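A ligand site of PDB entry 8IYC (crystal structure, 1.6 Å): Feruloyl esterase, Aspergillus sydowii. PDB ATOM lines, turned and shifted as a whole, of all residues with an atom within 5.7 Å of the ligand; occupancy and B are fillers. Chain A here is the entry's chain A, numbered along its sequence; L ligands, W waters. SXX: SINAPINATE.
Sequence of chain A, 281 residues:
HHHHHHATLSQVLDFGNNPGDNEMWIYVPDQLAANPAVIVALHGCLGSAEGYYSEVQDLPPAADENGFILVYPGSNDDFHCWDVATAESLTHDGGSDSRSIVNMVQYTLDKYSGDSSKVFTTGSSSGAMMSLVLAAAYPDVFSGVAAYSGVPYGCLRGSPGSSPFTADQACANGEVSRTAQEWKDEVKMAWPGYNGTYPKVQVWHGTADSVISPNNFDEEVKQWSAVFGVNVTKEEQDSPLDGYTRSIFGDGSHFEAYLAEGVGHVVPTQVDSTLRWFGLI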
ATOM      1  N   GLY A  44     -17.289   9.260  35.389  1.00  0.00           N
ATOM      2  CA  GLY A  44     -17.378  10.011  34.155  1.00  0.00           C
ATOM      3  C   GLY A  44     -16.388   9.528  33.108  1.00  0.00           C
ATOM      4  O   GLY A  44     -15.566   8.638  33.345  1.00  0.00           O
ATOM      5  N   CYS A  45     -16.477  10.137  31.918  1.00  0.00           N
ATOM      6  CA  CYS A  45     -15.564   9.804  30.828  1.00  0.00           C
ATOM      7  C   CYS A  45     -14.121   9.919  31.278  1.00  0.00           C
ATOM      8  O   CYS A  45     -13.757  10.776  32.084  1.00  0.00           O
ATOM      9  CB  CYS A  45     -15.797  10.727  29.623  1.00  0.00           C
ATOM     10  SG  CYS A  45     -17.120  10.198  28.465  1.00  0.00           S
ATOM     11  N   CYS A  81     -16.036   5.720  28.761  1.00  0.00           N
ATOM     12  CA  CYS A  81     -17.320   6.397  28.804  1.00  0.00           C
ATOM     13  C   CYS A  81     -18.455   5.385  28.783  1.00  0.00           C
ATOM     14  O   CYS A  81     -18.326   4.295  28.244  1.00  0.00           O
ATOM     15  CB  CYS A  81     -17.499   7.346  27.609  1.00  0.00           C
ATOM     16  SG  CYS A  81     -16.267   8.638  27.494  1.00  0.00           S
ATOM     17  N   VAL A  84     -24.300   5.496  25.926  1.00  0.00           N
ATOM     18  CA  VAL A  84     -25.642   6.072  26.006  1.00  0.00           C
ATOM     19  C   VAL A  84     -26.153   6.293  24.585  1.00  0.00           C
ATOM     20  O   VAL A  84     -26.998   7.167  24.338  1.00  0.00           O
ATOM     21  CB  VAL A  84     -25.645   7.374  26.830  1.00  0.00           C
ATOM     22  CG1 VAL A  84     -25.324   7.077  28.291  1.00  0.00           C
ATOM     23  CG2 VAL A  84     -24.698   8.415  26.244  1.00  0.00           C
ATOM     24  N   SER A 124     -21.741  11.198  37.531  1.00  0.00           N
ATOM     25  CA  SER A 124     -21.270  12.506  37.113  1.00  0.00           C
ATOM     26  C   SER A 124     -20.963  12.485  35.633  1.00  0.00           C
ATOM     27  O   SER A 124     -20.304  11.556  35.143  1.00  0.00           O
ATOM     28  CB  SER A 124     -20.034  12.929  37.918  1.00  0.00           C
ATOM     29  OG  SER A 124     -20.354  12.995  39.298  1.00  0.00           O
ATOM     30  N   SER A 125     -21.459  13.504  34.915  1.00  0.00           N
ATOM     31  CA  SER A 125     -21.280  13.628  33.473  1.00  0.00           C
ATOM     32  C   SER A 125     -21.700  12.345  32.762  1.00  0.00           C
ATOM     33  O   SER A 125     -22.876  11.988  32.782  1.00  0.00           O
ATOM     34  CB  SER A 125     -19.832  13.975  33.161  1.00  0.00           C
ATOM     35  OG  SER A 125     -19.496  15.212  33.728  1.00  0.00           O
ATOM     36  N   SER A 126     -20.757  11.646  32.123  1.00  0.00           N
ATOM     37  CA  SER A 126     -21.127  10.383  31.473  1.00  0.00           C
ATOM     38  C   SER A 126     -21.913   9.466  32.429  1.00  0.00           C
ATOM     39  O   SER A 126     -22.928   8.875  32.026  1.00  0.00           O
ATOM     40  CB  SER A 126     -19.888   9.659  30.955  1.00  0.00           C
ATOM     41  OG  SER A 126     -20.235   8.468  30.271  1.00  0.00           O
ATOM     42  N   GLY A 127     -21.496   9.379  33.696  1.00  0.00           N
ATOM     43  CA  GLY A 127     -22.232   8.579  34.657  1.00  0.00           C
ATOM     44  C   GLY A 127     -23.622   9.129  34.939  1.00  0.00           C
ATOM     45  O   GLY A 127     -24.546   8.372  35.236  1.00  0.00           O
ATOM     46  N   MET A 129     -25.348  10.750  32.639  1.00  0.00           N
ATOM     47  CA  MET A 129     -26.049  10.329  31.431  1.00  0.00           C
ATOM     48  C   MET A 129     -26.588   8.904  31.589  1.00  0.00           C
ATOM     49  O   MET A 129     -27.764   8.633  31.324  1.00  0.00           O
ATOM     50  CB  MET A 129     -25.054  10.426  30.296  1.00  0.00           C
ATOM     51  CG  MET A 129     -24.669  11.830  30.019  1.00  0.00           C
ATOM     52  SD  MET A 129     -23.622  11.968  28.567  1.00  0.00           S
ATOM     53  CE  MET A 129     -22.448  13.209  29.108  1.00  0.00           C
ATOM     54  N   LEU A 156     -28.285  11.145  22.702  1.00  0.00           N
ATOM     55  CA  LEU A 156     -27.212  10.541  21.909  1.00  0.00           C
ATOM     56  C   LEU A 156     -27.683   9.335  21.099  1.00  0.00           C
ATOM     57  O   LEU A 156     -26.849   8.623  20.542  1.00  0.00           O
ATOM     58  CB  LEU A 156     -26.044  10.123  22.815  1.00  0.00           C
ATOM     59  CG  LEU A 156     -25.007  11.144  23.309  1.00  0.00           C
ATOM     60  CD1 LEU A 156     -24.412  11.960  22.148  1.00  0.00           C
ATOM     61  CD2 LEU A 156     -25.555  12.059  24.412  1.00  0.00           C
ATOM     62  N   GLY A 161     -20.810   7.274  18.954  1.00  0.00           N
ATOM     63  CA  GLY A 161     -20.069   7.009  20.180  1.00  0.00           C
ATOM     64  C   GLY A 161     -20.665   7.829  21.300  1.00  0.00           C
ATOM     65  O   GLY A 161     -21.651   8.552  21.121  1.00  0.00           O
ATOM     66  N   SER A 162     -20.022   7.716  22.468  1.00  0.00           N
ATOM     67  CA  SER A 162     -20.498   8.397  23.673  1.00  0.00           C
ATOM     68  C   SER A 162     -19.388   9.155  24.381  1.00  0.00           C
ATOM     69  O   SER A 162     -19.501   9.417  25.583  1.00  0.00           O
ATOM     70  CB  SER A 162     -21.157   7.383  24.627  1.00  0.00           C
ATOM     71  OG  SER A 162     -22.281   6.783  24.018  1.00  0.00           O
ATOM     72  N   SER A 163     -18.330   9.538  23.677  1.00  0.00           N
ATOM     73  CA  SER A 163     -17.166  10.161  24.288  1.00  0.00           C
ATOM     74  C   SER A 163     -16.887  11.500  23.632  1.00  0.00           C
ATOM     75  O   SER A 163     -17.410  11.798  22.562  1.00  0.00           O
ATOM     76  CB  SER A 163     -15.950   9.231  24.165  1.00  0.00           C
ATOM     77  OG  SER A 163     -15.283   9.422  22.929  1.00  0.00           O
ATOM     78  N   PRO A 164     -16.051  12.346  24.267  1.00  0.00           N
ATOM     79  CA  PRO A 164     -15.657  13.608  23.605  1.00  0.00           C
ATOM     80  C   PRO A 164     -14.941  13.402  22.279  1.00  0.00           C
ATOM     81  O   PRO A 164     -14.802  14.374  21.525  1.00  0.00           O
ATOM     82  CB  PRO A 164     -14.711  14.262  24.621  1.00  0.00           C
ATOM     83  CG  PRO A 164     -14.977  13.568  25.921  1.00  0.00           C
ATOM     84  CD  PRO A 164     -15.441  12.196  25.591  1.00  0.00           C
ATOM     85  N   ALA A 167     -18.486  10.809  20.045  1.00  0.00           N
ATOM     86  CA  ALA A 167     -19.902  11.156  19.966  1.00  0.00           C
ATOM     87  C   ALA A 167     -20.130  12.251  18.928  1.00  0.00           C
ATOM     88  O   ALA A 167     -19.230  13.018  18.595  1.00  0.00           O
ATOM     89  CB  ALA A 167     -20.412  11.631  21.324  1.00  0.00           C
ATOM     90  N   ASP A 168     -21.338  12.280  18.377  1.00  0.00           N
ATOM     91  CA  ASP A 168     -21.856  13.529  17.844  1.00  0.00           C
ATOM     92  C   ASP A 168     -21.833  14.547  18.980  1.00  0.00           C
ATOM     93  O   ASP A 168     -22.410  14.302  20.046  1.00  0.00           O
ATOM     94  CB  ASP A 168     -23.278  13.308  17.326  1.00  0.00           C
ATOM     95  CG  ASP A 168     -23.902  14.551  16.752  1.00  0.00           C
ATOM     96  OD1 ASP A 168     -23.366  15.670  16.946  1.00  0.00           O
ATOM     97  OD2 ASP A 168     -24.961  14.407  16.089  1.00  0.00           O
ATOM     98  N   GLN A 169     -21.158  15.672  18.766  1.00  0.00           N
ATOM     99  CA  GLN A 169     -20.979  16.649  19.841  1.00  0.00           C
ATOM    100  C   GLN A 169     -22.165  17.574  20.036  1.00  0.00           C
ATOM    101  O   GLN A 169     -22.118  18.431  20.933  1.00  0.00           O
ATOM    102  CB  GLN A 169     -19.726  17.487  19.583  1.00  0.00           C
ATOM    103  CG  GLN A 169     -18.435  16.669  19.596  1.00  0.00           C
ATOM    104  CD  GLN A 169     -18.273  15.863  20.876  1.00  0.00           C
ATOM    105  OE1 GLN A 169     -18.286  16.433  21.970  1.00  0.00           O
ATOM    106  NE2 GLN A 169     -18.123  14.545  20.751  1.00  0.00           N
ATOM    107  N   ALA A 172     -23.446  17.507  23.852  1.00  0.00           N
ATOM    108  CA  ALA A 172     -22.546  18.127  24.823  1.00  0.00           C
ATOM    109  C   ALA A 172     -22.421  19.626  24.592  1.00  0.00           C
ATOM    110  O   ALA A 172     -22.230  20.387  25.542  1.00  0.00           O
ATOM    111  CB  ALA A 172     -21.164  17.464  24.769  1.00  0.00           C
ATOM    112  N   VAL A 211     -17.828  21.679  29.551  1.00  0.00           N
ATOM    113  CA  VAL A 211     -17.757  20.337  28.974  1.00  0.00           C
ATOM    114  C   VAL A 211     -19.141  19.899  28.486  1.00  0.00           C
ATOM    115  O   VAL A 211     -19.309  19.537  27.317  1.00  0.00           O
ATOM    116  CB  VAL A 211     -17.169  19.348  29.993  1.00  0.00           C
ATOM    117  CG1 VAL A 211     -17.200  17.927  29.435  1.00  0.00           C
ATOM    118  CG2 VAL A 211     -15.751  19.733  30.388  1.00  0.00           C
ATOM    119  N   ILE A 212     -20.124  19.887  29.376  1.00  0.00           N
ATOM    120  CA  ILE A 212     -21.513  19.567  29.041  1.00  0.00           C
ATOM    121  C   ILE A 212     -22.323  20.846  29.222  1.00  0.00           C
ATOM    122  O   ILE A 212     -22.459  21.343  30.346  1.00  0.00           O
ATOM    123  CB  ILE A 212     -22.071  18.434  29.905  1.00  0.00           C
ATOM    124  CG1 ILE A 212     -21.212  17.175  29.784  1.00  0.00           C
ATOM    125  CG2 ILE A 212     -23.543  18.162  29.545  1.00  0.00           C
ATOM    126  CD1 ILE A 212     -21.217  16.553  28.417  1.00  0.00           C
ATOM    127  N   HIS A 265     -17.831  21.989  35.254  1.00  0.00           N
ATOM    128  CA  HIS A 265     -17.801  20.531  35.154  1.00  0.00           C
ATOM    129  C   HIS A 265     -16.978  19.979  36.304  1.00  0.00           C
ATOM    130  O   HIS A 265     -15.770  20.218  36.357  1.00  0.00           O
ATOM    131  CB  HIS A 265     -17.205  20.171  33.799  1.00  0.00           C
ATOM    132  CG  HIS A 265     -16.717  18.767  33.665  1.00  0.00           C
ATOM    133  ND1 HIS A 265     -17.474  17.756  33.131  1.00  0.00           N
ATOM    134  CD2 HIS A 265     -15.505  18.215  33.945  1.00  0.00           C
ATOM    135  CE1 HIS A 265     -16.777  16.636  33.115  1.00  0.00           C
ATOM    136  NE2 HIS A 265     -15.578  16.884  33.602  1.00  0.00           N
ATOM    137  N   VAL A 266     -17.582  19.266  37.262  1.00  0.00           N
ATOM    138  CA  VAL A 266     -19.004  18.955  37.406  1.00  0.00           C
ATOM    139  C   VAL A 266     -19.521  19.572  38.708  1.00  0.00           C
ATOM    140  O   VAL A 266     -18.732  20.070  39.515  1.00  0.00           O
ATOM    141  CB  VAL A 266     -19.274  17.415  37.451  1.00  0.00           C
ATOM    142  CG1 VAL A 266     -18.857  16.742  36.189  1.00  0.00           C
ATOM    143  CG2 VAL A 266     -18.573  16.773  38.663  1.00  0.00           C
HETATM  144  C1  SXX L   1     -19.327  14.365  24.815  1.00  0.00           C
HETATM  145  C2  SXX L   1     -18.434  15.129  25.555  1.00  0.00           C
HETATM  146  C3  SXX L   1     -18.175  14.789  26.868  1.00  0.00           C
HETATM  147  C4  SXX L   1     -18.812  13.693  27.418  1.00  0.00           C
HETATM  148  C5  SXX L   1     -19.697  12.924  26.667  1.00  0.00           C
HETATM  149  C6  SXX L   1     -19.955  13.279  25.368  1.00  0.00           C
HETATM  150  O7  SXX L   1     -19.619  14.672  23.483  1.00  0.00           O
HETATM  151  O8  SXX L   1     -20.842  12.554  24.559  1.00  0.00           O
HETATM  152  O9  SXX L   1     -17.819  16.234  24.927  1.00  0.00           O
HETATM  153  C10 SXX L   1     -18.542  13.266  28.860  1.00  0.00           C
HETATM  154  C11 SXX L   1     -17.686  13.911  29.596  1.00  0.00           C
HETATM  155  C12 SXX L   1     -17.438  13.388  31.009  1.00  0.00           C
HETATM  156  O13 SXX L   1     -16.635  13.989  31.767  1.00  0.00           O
HETATM  157  O14 SXX L   1     -18.026  12.336  31.395  1.00  0.00           O
HETATM  158  C15 SXX L   1     -17.058  17.088  25.720  1.00  0.00           C
HETATM  159  C14 SXX L   1     -21.751  11.765  25.257  1.00  0.00           C
HETATM  160  O   HOH W   1     -15.668  13.380  33.956  1.00  0.00           O
HETATM  161  O   HOH W   2     -22.402  15.143  22.703  1.00  0.00           O
HETATM  162  O   HOH W   3     -14.229  15.077  30.473  1.00  0.00           O
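Water W2 lies within hydrogen-bond range of O of Asp 168 (2.8 Å), N of Ala 172 (2.8 Å) and O7 of the ligand (2.9 Å).
Gly 44 touches the ligand.
Ser 125 touches the ligand.
CE of Met 129 touches C5 of the ligand, 3.7 Å away.
Leu 156 touches the ligand (CG to C14, 3.8 Å).
O of Ser 162 touches C14 of the ligand, at 3.3 Å.
Ser 163 touches the ligand (O to O7, 3.7 Å).
Pro 164 touches the ligand.
Ala 167 touches the ligand.
CB of Ala 172 touches O7 of the ligand, at 3.4 Å.
O of Val 211 touches C15 of the ligand, at 3.7 Å.
Ile 212 touches the ligand.
CE1 of His 265 touches O13 of the ligand, 3.0 Å away.
Hydrophobic or aromatic side chains that line the ligand: Met 129, Leu 156, Pro 164, Ala 167, Ala 172, Val 211, Ile 212 and His 265.
The nearest printed residue that does not touch the ligand is Asp 168 (4.4 Å).
An oxygen (O7) of the ligand lies within hydrogen-bond range of the side-chain amide oxygen (OE1) of Gln 169 (2.7 Å).
N of Cys 45 is in hydrogen-bond range of O14 of the ligand (2.7 Å).
N of Ser 126 lies within hydrogen-bond range of O14 of the ligand, at 2.9 Å.
The side-chain sulfur of Cys 45 is disulfide-bonded to the side-chain sulfur of Cys 81, at 2.0 Å.
OG of Ser 125 lies close to ND1 of His 265 (3.3 Å).
The side-chain hydroxyl of Ser 162 lies within hydrogen-bond range of the backbone NH of Val 84, 3.1 Å away.
The side-chain amide nitrogen (NE2) of Gln 169 sits at hydrogen-bond distance from the backbone carbonyl oxygen (O) of Ala 167 (2.9 Å).
The backbone carbonyl oxygen of Pro 164 is in hydrogen-bond range of the side-chain amide nitrogen of Gln 169 (3.4 Å).
O of Ser 163 sits at hydrogen-bond distance from NE2 of Gln 169, at 3.4 Å.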
